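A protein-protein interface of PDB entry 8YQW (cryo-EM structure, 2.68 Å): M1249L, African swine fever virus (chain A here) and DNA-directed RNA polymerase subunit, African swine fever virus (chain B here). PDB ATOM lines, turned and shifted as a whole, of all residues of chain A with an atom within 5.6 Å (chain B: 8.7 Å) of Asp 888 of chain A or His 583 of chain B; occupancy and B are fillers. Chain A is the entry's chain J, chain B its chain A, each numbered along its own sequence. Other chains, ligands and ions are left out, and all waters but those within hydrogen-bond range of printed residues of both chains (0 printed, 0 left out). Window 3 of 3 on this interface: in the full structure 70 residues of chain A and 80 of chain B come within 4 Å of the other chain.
O of Pro 580 of chain B is in hydrogen-bond range of OH of Tyr 864 of chain A, 2.5 Å away.
A ring nitrogen (ND1) of His 583 of chain B sits close to the backbone carbonyl oxygen (O) of Asp 888 of chain A (3.5 Å).
NE2 of His 583 of chain B sits close to O of Tyr 891 of chain A (3.1 Å).
Of chain B, only His 583 (3.3 Å) comes within 4 Å of Asp 888 of chain A.
His 583 of chain B touches three residues of chain A.
Printed residues of chain B within 4 Å of Val 883 of chain A: Ala 579 (3.3 Å) and Pro 580 (3.8 Å).
Printed residues of chain B within 4 Å of Asn 889 of chain A: His 583.
Of the printed residues of chain B, Tyr 891 of chain A touches His 583.
Printed residues of chain A within 4 Å of Pro 580 of chain B: Tyr 864 (2.5 Å) and Val 883 (3.8 Å).
Of the printed residues of chain A, Ala 579 of chain B touches Val 883 (3.3 Å).
Asn 724 of chain B touches none of the printed residues of chain A.
Ala 892 of chain A touches none of the printed residues of chain B.
The nearest residue of chain B that does not touch Asp 888 of chain A is Tyr 584 of chain B (6.4 Å).
The nearest residue of chain A that does not touch His 583 of chain B is Ile 887 of chain A (4.5 Å).
The nearest printed residue of chain B that does not touch Tyr 864 of chain A is Ala 579 of chain B (4.4 Å).
O of Ala 579 of chain B touches CG1 of Val 883 of chain A (3.3 Å).
Val 883 of chain A touches Pro 580 of chain B.
His 583 of chain B touches Asn 889 of chain A (ND1 to CA, 3.8 Å).
Hydrophobic or aromatic side chains of chain A within 4 Å of the printed part of chain B: Tyr 864 and Val 883.
Of the 18 printed residues of chain B, 3 touch a printed residue of chain A.
Printed residues of chain B that touch a printed residue of chain A: Ala 579, Pro 580 and His 583.
Among the printed residues, no Asp or Glu carboxylate lies within 4 Å of a Lys or Arg side-chain nitrogen of the other chain.
OH of Tyr 891 of chain A sits at hydrogen-bond distance from NE2 of Gln 871 of chain A (3.4 Å).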
ATOM      1  N   TYR A 864      35.794  16.895  27.483  1.00  0.00           N
ATOM      2  CA  TYR A 864      34.902  17.785  28.209  1.00  0.00           C
ATOM      3  C   TYR A 864      35.265  17.761  29.683  1.00  0.00           C
ATOM      4  O   TYR A 864      35.407  16.686  30.274  1.00  0.00           O
ATOM      5  CB  TYR A 864      33.441  17.371  28.026  1.00  0.00           C
ATOM      6  CG  TYR A 864      32.915  17.596  26.632  1.00  0.00           C
ATOM      7  CD1 TYR A 864      33.073  16.634  25.648  1.00  0.00           C
ATOM      8  CD2 TYR A 864      32.257  18.768  26.300  1.00  0.00           C
ATOM      9  CE1 TYR A 864      32.595  16.835  24.377  1.00  0.00           C
ATOM     10  CE2 TYR A 864      31.776  18.977  25.032  1.00  0.00           C
ATOM     11  CZ  TYR A 864      31.948  18.008  24.074  1.00  0.00           C
ATOM     12  OH  TYR A 864      31.469  18.216  22.809  1.00  0.00           O
ATOM     13  N   GLN A 871      31.144  18.041  40.423  1.00  0.00           N
ATOM     14  CA  GLN A 871      30.636  17.129  39.407  1.00  0.00           C
ATOM     15  C   GLN A 871      31.652  16.033  39.111  1.00  0.00           C
ATOM     16  O   GLN A 871      32.857  16.281  39.032  1.00  0.00           O
ATOM     17  CB  GLN A 871      30.298  17.903  38.131  1.00  0.00           C
ATOM     18  CG  GLN A 871      29.783  17.042  36.990  1.00  0.00           C
ATOM     19  CD  GLN A 871      28.272  16.974  36.945  1.00  0.00           C
ATOM     20  OE1 GLN A 871      27.587  17.941  37.278  1.00  0.00           O
ATOM     21  NE2 GLN A 871      27.740  15.830  36.528  1.00  0.00           N
ATOM     22  N   VAL A 883      28.441  12.672  21.576  1.00  0.00           N
ATOM     23  CA  VAL A 883      28.335  13.890  22.375  1.00  0.00           C
ATOM     24  C   VAL A 883      26.917  14.066  22.896  1.00  0.00           C
ATOM     25  O   VAL A 883      26.705  14.391  24.070  1.00  0.00           O
ATOM     26  CB  VAL A 883      28.789  15.109  21.552  1.00  0.00           C
ATOM     27  CG1 VAL A 883      28.525  16.389  22.318  1.00  0.00           C
ATOM     28  CG2 VAL A 883      30.260  14.990  21.193  1.00  0.00           C
ATOM     29  N   LYS A 886      26.304  11.494  25.986  1.00  0.00           N
ATOM     30  CA  LYS A 886      27.080  11.440  27.216  1.00  0.00           C
ATOM     31  C   LYS A 886      27.419  12.797  27.813  1.00  0.00           C
ATOM     32  O   LYS A 886      27.951  12.835  28.927  1.00  0.00           O
ATOM     33  CB  LYS A 886      28.386  10.666  26.987  1.00  0.00           C
ATOM     34  CG  LYS A 886      28.176   9.223  26.561  1.00  0.00           C
ATOM     35  CD  LYS A 886      29.489   8.480  26.430  1.00  0.00           C
ATOM     36  CE  LYS A 886      29.255   7.026  26.056  1.00  0.00           C
ATOM     37  NZ  LYS A 886      28.627   6.892  24.713  1.00  0.00           N
ATOM     38  N   ILE A 887      27.136  13.901  27.128  1.00  0.00           N
ATOM     39  CA  ILE A 887      27.523  15.231  27.578  1.00  0.00           C
ATOM     40  C   ILE A 887      26.268  16.079  27.737  1.00  0.00           C
ATOM     41  O   ILE A 887      25.426  16.125  26.833  1.00  0.00           O
ATOM     42  CB  ILE A 887      28.510  15.896  26.601  1.00  0.00           C
ATOM     43  CG1 ILE A 887      29.685  14.965  26.310  1.00  0.00           C
ATOM     44  CG2 ILE A 887      29.012  17.210  27.162  1.00  0.00           C
ATOM     45  CD1 ILE A 887      30.516  14.628  27.528  1.00  0.00           C
ATOM     46  N   ASP A 888      26.145  16.738  28.883  1.00  0.00           N
ATOM     47  CA  ASP A 888      25.081  17.696  29.150  1.00  0.00           C
ATOM     48  C   ASP A 888      25.702  19.067  29.423  1.00  0.00           C
ATOM     49  O   ASP A 888      26.910  19.263  29.275  1.00  0.00           O
ATOM     50  CB  ASP A 888      24.199  17.220  30.308  1.00  0.00           C
ATOM     51  CG  ASP A 888      24.998  16.864  31.542  1.00  0.00           C
ATOM     52  OD1 ASP A 888      26.241  16.910  31.481  1.00  0.00           O
ATOM     53  OD2 ASP A 888      24.382  16.531  32.576  1.00  0.00           O
ATOM     54  N   ASN A 889      24.865  20.022  29.826  1.00  0.00           N
ATOM     55  CA  ASN A 889      25.345  21.379  30.065  1.00  0.00           C
ATOM     56  C   ASN A 889      26.191  21.502  31.325  1.00  0.00           C
ATOM     57  O   ASN A 889      26.681  22.600  31.611  1.00  0.00           O
ATOM     58  CB  ASN A 889      24.166  22.352  30.133  1.00  0.00           C
ATOM     59  CG  ASN A 889      23.035  21.839  30.994  1.00  0.00           C
ATOM     60  OD1 ASN A 889      23.026  20.677  31.402  1.00  0.00           O
ATOM     61  ND2 ASN A 889      22.070  22.705  31.278  1.00  0.00           N
ATOM     62  N   HIS A 890      26.370  20.421  32.083  1.00  0.00           N
ATOM     63  CA  HIS A 890      27.273  20.423  33.225  1.00  0.00           C
ATOM     64  C   HIS A 890      28.739  20.345  32.822  1.00  0.00           C
ATOM     65  O   HIS A 890      29.610  20.502  33.684  1.00  0.00           O
ATOM     66  CB  HIS A 890      26.942  19.260  34.162  1.00  0.00           C
ATOM     67  CG  HIS A 890      25.638  19.416  34.881  1.00  0.00           C
ATOM     68  ND1 HIS A 890      25.021  18.373  35.538  1.00  0.00           N
ATOM     69  CD2 HIS A 890      24.833  20.492  35.044  1.00  0.00           C
ATOM     70  CE1 HIS A 890      23.894  18.801  36.075  1.00  0.00           C
ATOM     71  NE2 HIS A 890      23.756  20.083  35.791  1.00  0.00           N
ATOM     72  N   TYR A 891      29.031  20.106  31.547  1.00  0.00           N
ATOM     73  CA  TYR A 891      30.392  19.981  31.053  1.00  0.00           C
ATOM     74  C   TYR A 891      30.634  20.994  29.942  1.00  0.00           C
ATOM     75  O   TYR A 891      29.702  21.451  29.278  1.00  0.00           O
ATOM     76  CB  TYR A 891      30.666  18.565  30.535  1.00  0.00           C
ATOM     77  CG  TYR A 891      30.520  17.494  31.589  1.00  0.00           C
ATOM     78  CD1 TYR A 891      29.289  16.910  31.844  1.00  0.00           C
ATOM     79  CD2 TYR A 891      31.611  17.064  32.326  1.00  0.00           C
ATOM     80  CE1 TYR A 891      29.150  15.931  32.805  1.00  0.00           C
ATOM     81  CE2 TYR A 891      31.481  16.087  33.289  1.00  0.00           C
ATOM     82  CZ  TYR A 891      30.248  15.525  33.525  1.00  0.00           C
ATOM     83  OH  TYR A 891      30.115  14.550  34.483  1.00  0.00           O
ATOM     84  N   ALA A 892      31.902  21.349  29.752  1.00  0.00           N
ATOM     85  CA  ALA A 892      32.305  22.261  28.693  1.00  0.00           C
ATOM     86  C   ALA A 892      33.474  21.663  27.925  1.00  0.00           C
ATOM     87  O   ALA A 892      34.322  20.970  28.494  1.00  0.00           O
ATOM     88  CB  ALA A 892      32.690  23.636  29.248  1.00  0.00           C
ATOM     89  N   ASN B 514      13.234  26.273  25.684  1.00  0.00           N
ATOM     90  CA  ASN B 514      13.752  27.314  26.556  1.00  0.00           C
ATOM     91  C   ASN B 514      14.091  28.558  25.749  1.00  0.00           C
ATOM     92  O   ASN B 514      14.308  28.496  24.538  1.00  0.00           O
ATOM     93  CB  ASN B 514      14.996  26.847  27.318  1.00  0.00           C
ATOM     94  CG  ASN B 514      14.672  25.857  28.414  1.00  0.00           C
ATOM     95  OD1 ASN B 514      15.133  24.718  28.391  1.00  0.00           O
ATOM     96  ND2 ASN B 514      13.877  26.287  29.382  1.00  0.00           N
ATOM     97  N   TRP B 573      17.070  21.280  13.368  1.00  0.00           N
ATOM     98  CA  TRP B 573      17.847  21.946  14.406  1.00  0.00           C
ATOM     99  C   TRP B 573      18.978  21.059  14.907  1.00  0.00           C
ATOM    100  O   TRP B 573      20.089  21.541  15.150  1.00  0.00           O
ATOM    101  CB  TRP B 573      16.918  22.356  15.550  1.00  0.00           C
ATOM    102  CG  TRP B 573      17.595  22.953  16.742  1.00  0.00           C
ATOM    103  CD1 TRP B 573      17.714  22.393  17.975  1.00  0.00           C
ATOM    104  CD2 TRP B 573      18.234  24.231  16.817  1.00  0.00           C
ATOM    105  NE1 TRP B 573      18.390  23.238  18.815  1.00  0.00           N
ATOM    106  CE2 TRP B 573      18.721  24.375  18.128  1.00  0.00           C
ATOM    107  CE3 TRP B 573      18.443  25.267  15.904  1.00  0.00           C
ATOM    108  CZ2 TRP B 573      19.404  25.510  18.549  1.00  0.00           C
ATOM    109  CZ3 TRP B 573      19.119  26.392  16.324  1.00  0.00           C
ATOM    110  CH2 TRP B 573      19.592  26.506  17.634  1.00  0.00           C
ATOM    111  N   TYR B 574      18.727  19.761  15.051  1.00  0.00           N
ATOM    112  CA  TYR B 574      19.762  18.852  15.526  1.00  0.00           C
ATOM    113  C   TYR B 574      20.678  18.444  14.381  1.00  0.00           C
ATOM    114  O   TYR B 574      20.215  17.933  13.357  1.00  0.00           O
ATOM    115  CB  TYR B 574      19.169  17.605  16.169  1.00  0.00           C
ATOM    116  CG  TYR B 574      20.260  16.658  16.598  1.00  0.00           C
ATOM    117  CD1 TYR B 574      21.181  17.031  17.563  1.00  0.00           C
ATOM    118  CD2 TYR B 574      20.405  15.415  16.003  1.00  0.00           C
ATOM    119  CE1 TYR B 574      22.193  16.186  17.946  1.00  0.00           C
ATOM    120  CE2 TYR B 574      21.419  14.560  16.380  1.00  0.00           C
ATOM    121  CZ  TYR B 574      22.311  14.953  17.353  1.00  0.00           C
ATOM    122  OH  TYR B 574      23.325  14.108  17.739  1.00  0.00           O
ATOM    123  N   TYR B 578      27.041  20.360  14.730  1.00  0.00           N
ATOM    124  CA  TYR B 578      27.058  21.314  15.830  1.00  0.00           C
ATOM    125  C   TYR B 578      27.086  20.657  17.202  1.00  0.00           C
ATOM    126  O   TYR B 578      27.359  21.345  18.189  1.00  0.00           O
ATOM    127  CB  TYR B 578      25.834  22.231  15.768  1.00  0.00           C
ATOM    128  CG  TYR B 578      25.621  22.926  14.450  1.00  0.00           C
ATOM    129  CD1 TYR B 578      26.674  23.510  13.768  1.00  0.00           C
ATOM    130  CD2 TYR B 578      24.357  23.005  13.892  1.00  0.00           C
ATOM    131  CE1 TYR B 578      26.473  24.146  12.567  1.00  0.00           C
ATOM    132  CE2 TYR B 578      24.147  23.639  12.694  1.00  0.00           C
ATOM    133  CZ  TYR B 578      25.206  24.207  12.035  1.00  0.00           C
ATOM    134  OH  TYR B 578      24.994  24.842  10.837  1.00  0.00           O
ATOM    135  N   ALA B 579      26.805  19.359  17.288  1.00  0.00           N
ATOM    136  CA  ALA B 579      26.651  18.715  18.590  1.00  0.00           C
ATOM    137  C   ALA B 579      27.861  18.854  19.509  1.00  0.00           C
ATOM    138  O   ALA B 579      27.654  19.111  20.707  1.00  0.00           O
ATOM    139  CB  ALA B 579      26.293  17.237  18.392  1.00  0.00           C
ATOM    140  N   PRO B 580      29.108  18.684  19.056  1.00  0.00           N
ATOM    141  CA  PRO B 580      30.233  18.832  19.992  1.00  0.00           C
ATOM    142  C   PRO B 580      30.339  20.210  20.611  1.00  0.00           C
ATOM    143  O   PRO B 580      30.823  20.335  21.741  1.00  0.00           O
ATOM    144  CB  PRO B 580      31.454  18.524  19.119  1.00  0.00           C
ATOM    145  CG  PRO B 580      30.936  17.725  18.018  1.00  0.00           C
ATOM    146  CD  PRO B 580      29.582  18.256  17.728  1.00  0.00           C
ATOM    147  N   TYR B 581      29.900  21.249  19.907  1.00  0.00           N
ATOM    148  CA  TYR B 581      30.170  22.620  20.305  1.00  0.00           C
ATOM    149  C   TYR B 581      28.938  23.319  20.853  1.00  0.00           C
ATOM    150  O   TYR B 581      29.011  24.499  21.208  1.00  0.00           O
ATOM    151  CB  TYR B 581      30.728  23.395  19.114  1.00  0.00           C
ATOM    152  CG  TYR B 581      31.809  22.643  18.379  1.00  0.00           C
ATOM    153  CD1 TYR B 581      33.068  22.480  18.926  1.00  0.00           C
ATOM    154  CD2 TYR B 581      31.562  22.091  17.133  1.00  0.00           C
ATOM    155  CE1 TYR B 581      34.047  21.781  18.254  1.00  0.00           C
ATOM    156  CE2 TYR B 581      32.531  21.400  16.456  1.00  0.00           C
ATOM    157  CZ  TYR B 581      33.773  21.248  17.017  1.00  0.00           C
ATOM    158  OH  TYR B 581      34.740  20.554  16.330  1.00  0.00           O
ATOM    159  N   MET B 582      27.811  22.620  20.928  1.00  0.00           N
ATOM    160  CA  MET B 582      26.558  23.173  21.410  1.00  0.00           C
ATOM    161  C   MET B 582      25.938  22.212  22.410  1.00  0.00           C
ATOM    162  O   MET B 582      26.101  20.995  22.303  1.00  0.00           O
ATOM    163  CB  MET B 582      25.570  23.412  20.263  1.00  0.00           C
ATOM    164  CG  MET B 582      24.370  24.243  20.649  1.00  0.00           C
ATOM    165  SD  MET B 582      22.935  23.895  19.631  1.00  0.00           S
ATOM    166  CE  MET B 582      23.602  24.248  18.021  1.00  0.00           C
ATOM    167  N   HIS B 583      25.228  22.764  23.387  1.00  0.00           N
ATOM    168  CA  HIS B 583      24.461  21.954  24.328  1.00  0.00           C
ATOM    169  C   HIS B 583      23.023  21.890  23.831  1.00  0.00           C
ATOM    170  O   HIS B 583      22.219  22.785  24.102  1.00  0.00           O
ATOM    171  CB  HIS B 583      24.548  22.525  25.737  1.00  0.00           C
ATOM    172  CG  HIS B 583      25.924  22.477  26.321  1.00  0.00           C
ATOM    173  ND1 HIS B 583      26.613  21.297  26.499  1.00  0.00           N
ATOM    174  CD2 HIS B 583      26.742  23.461  26.763  1.00  0.00           C
ATOM    175  CE1 HIS B 583      27.795  21.556  27.026  1.00  0.00           C
ATOM    176  NE2 HIS B 583      27.899  22.862  27.197  1.00  0.00           N
ATOM    177  N   TYR B 584      22.703  20.837  23.089  1.00  0.00           N
ATOM    178  CA  TYR B 584      21.338  20.630  22.632  1.00  0.00           C
ATOM    179  C   TYR B 584      20.440  20.272  23.806  1.00  0.00           C
ATOM    180  O   TYR B 584      20.843  19.552  24.722  1.00  0.00           O
ATOM    181  CB  TYR B 584      21.288  19.522  21.586  1.00  0.00           C
ATOM    182  CG  TYR B 584      21.558  19.982  20.177  1.00  0.00           C
ATOM    183  CD1 TYR B 584      20.622  20.721  19.479  1.00  0.00           C
ATOM    184  CD2 TYR B 584      22.749  19.673  19.542  1.00  0.00           C
ATOM    185  CE1 TYR B 584      20.862  21.138  18.193  1.00  0.00           C
ATOM    186  CE2 TYR B 584      22.998  20.090  18.255  1.00  0.00           C
ATOM    187  CZ  TYR B 584      22.051  20.823  17.586  1.00  0.00           C
ATOM    188  OH  TYR B 584      22.287  21.245  16.302  1.00  0.00           O
ATOM    189  N   ASN B 585      19.214  20.782  23.777  1.00  0.00           N
ATOM    190  CA  ASN B 585      18.216  20.399  24.761  1.00  0.00           C
ATOM    191  C   ASN B 585      17.578  19.086  24.333  1.00  0.00           C
ATOM    192  O   ASN B 585      17.188  18.925  23.173  1.00  0.00           O
ATOM    193  CB  ASN B 585      17.163  21.496  24.909  1.00  0.00           C
ATOM    194  CG  ASN B 585      16.317  21.332  26.155  1.00  0.00           C
ATOM    195  OD1 ASN B 585      16.072  20.220  26.614  1.00  0.00           O
ATOM    196  ND2 ASN B 585      15.880  22.446  26.719  1.00  0.00           N
ATOM    197  N   LYS B 586      17.477  18.144  25.270  1.00  0.00           N
ATOM    198  CA  LYS B 586      16.962  16.821  24.945  1.00  0.00           C
ATOM    199  C   LYS B 586      15.480  16.829  24.600  1.00  0.00           C
ATOM    200  O   LYS B 586      14.975  15.819  24.100  1.00  0.00           O
ATOM    201  CB  LYS B 586      17.220  15.863  26.103  1.00  0.00           C
ATOM    202  CG  LYS B 586      18.592  15.212  26.068  1.00  0.00           C
ATOM    203  CD  LYS B 586      18.672  14.141  24.995  1.00  0.00           C
ATOM    204  CE  LYS B 586      19.945  13.321  25.133  1.00  0.00           C
ATOM    205  NZ  LYS B 586      19.881  12.052  24.357  1.00  0.00           N
ATOM    206  N   ASP B 588      14.241  19.138  22.476  1.00  0.00           N
ATOM    207  CA  ASP B 588      14.142  19.834  21.204  1.00  0.00           C
ATOM    208  C   ASP B 588      14.598  19.006  20.014  1.00  0.00           C
ATOM    209  O   ASP B 588      14.276  19.363  18.879  1.00  0.00           O
ATOM    210  CB  ASP B 588      14.966  21.128  21.238  1.00  0.00           C
ATOM    211  CG  ASP B 588      14.362  22.180  22.135  1.00  0.00           C
ATOM    212  OD1 ASP B 588      13.132  22.151  22.334  1.00  0.00           O
ATOM    213  OD2 ASP B 588      15.114  23.037  22.640  1.00  0.00           O
ATOM    214  N   ILE B 589      15.328  17.921  20.241  1.00  0.00           N
ATOM    215  CA  ILE B 589      15.957  17.170  19.168  1.00  0.00           C
ATOM    216  C   ILE B 589      15.125  15.951  18.770  1.00  0.00           C
ATOM    217  O   ILE B 589      15.618  15.068  18.075  1.00  0.00           O
ATOM    218  CB  ILE B 589      17.389  16.765  19.539  1.00  0.00           C
ATOM    219  CG1 ILE B 589      17.373  15.895  20.794  1.00  0.00           C
ATOM    220  CG2 ILE B 589      18.236  17.995  19.769  1.00  0.00           C
ATOM    221  CD1 ILE B 589      18.713  15.325  21.157  1.00  0.00           C
ATOM    222  N   MET B 720      31.781  28.278  16.498  1.00  0.00           N
ATOM    223  CA  MET B 720      30.757  28.040  17.505  1.00  0.00           C
ATOM    224  C   MET B 720      31.128  28.585  18.876  1.00  0.00           C
ATOM    225  O   MET B 720      30.233  28.775  19.705  1.00  0.00           O
ATOM    226  CB  MET B 720      30.459  26.544  17.618  1.00  0.00           C
ATOM    227  CG  MET B 720      29.794  25.933  16.395  1.00  0.00           C
ATOM    228  SD  MET B 720      28.200  26.665  16.003  1.00  0.00           S
ATOM    229  CE  MET B 720      27.238  26.116  17.404  1.00  0.00           C
ATOM    230  N   ASN B 724      26.360  32.510  20.329  1.00  0.00           N
ATOM    231  CA  ASN B 724      25.400  31.922  21.251  1.00  0.00           C
ATOM    232  C   ASN B 724      24.225  31.396  20.443  1.00  0.00           C
ATOM    233  O   ASN B 724      23.475  32.195  19.865  1.00  0.00           O
ATOM    234  CB  ASN B 724      24.930  32.954  22.276  1.00  0.00           C
ATOM    235  CG  ASN B 724      24.192  32.326  23.440  1.00  0.00           C
ATOM    236  OD1 ASN B 724      23.973  31.119  23.474  1.00  0.00           O
ATOM    237  ND2 ASN B 724      23.814  33.147  24.407  1.00  0.00           N
ATOM    238  N   PRO B 725      24.031  30.078  20.355  1.00  0.00           N
ATOM    239  CA  PRO B 725      22.927  29.556  19.534  1.00  0.00           C
ATOM    240  C   PRO B 725      21.555  30.025  19.981  1.00  0.00           C
ATOM    241  O   PRO B 725      20.639  30.101  19.155  1.00  0.00           O
ATOM    242  CB  PRO B 725      23.082  28.037  19.677  1.00  0.00           C
ATOM    243  CG  PRO B 725      24.507  27.836  20.051  1.00  0.00           C
ATOM    244  CD  PRO B 725      24.854  28.998  20.920  1.00  0.00           C
ATOM    245  N   GLU B 726      21.380  30.340  21.265  1.00  0.00           N
ATOM    246  CA  GLU B 726      20.090  30.812  21.745  1.00  0.00           C
ATOM    247  C   GLU B 726      19.734  32.194  21.219  1.00  0.00           C
ATOM    248  O   GLU B 726      18.547  32.491  21.053  1.00  0.00           O
ATOM    249  CB  GLU B 726      20.066  30.835  23.272  1.00  0.00           C
ATOM    250  CG  GLU B 726      20.124  29.472  23.916  1.00  0.00           C
ATOM    251  CD  GLU B 726      19.949  29.542  25.417  1.00  0.00           C
ATOM    252  OE1 GLU B 726      19.895  30.667  25.955  1.00  0.00           O
ATOM    253  OE2 GLU B 726      19.857  28.474  26.057  1.00  0.00           O
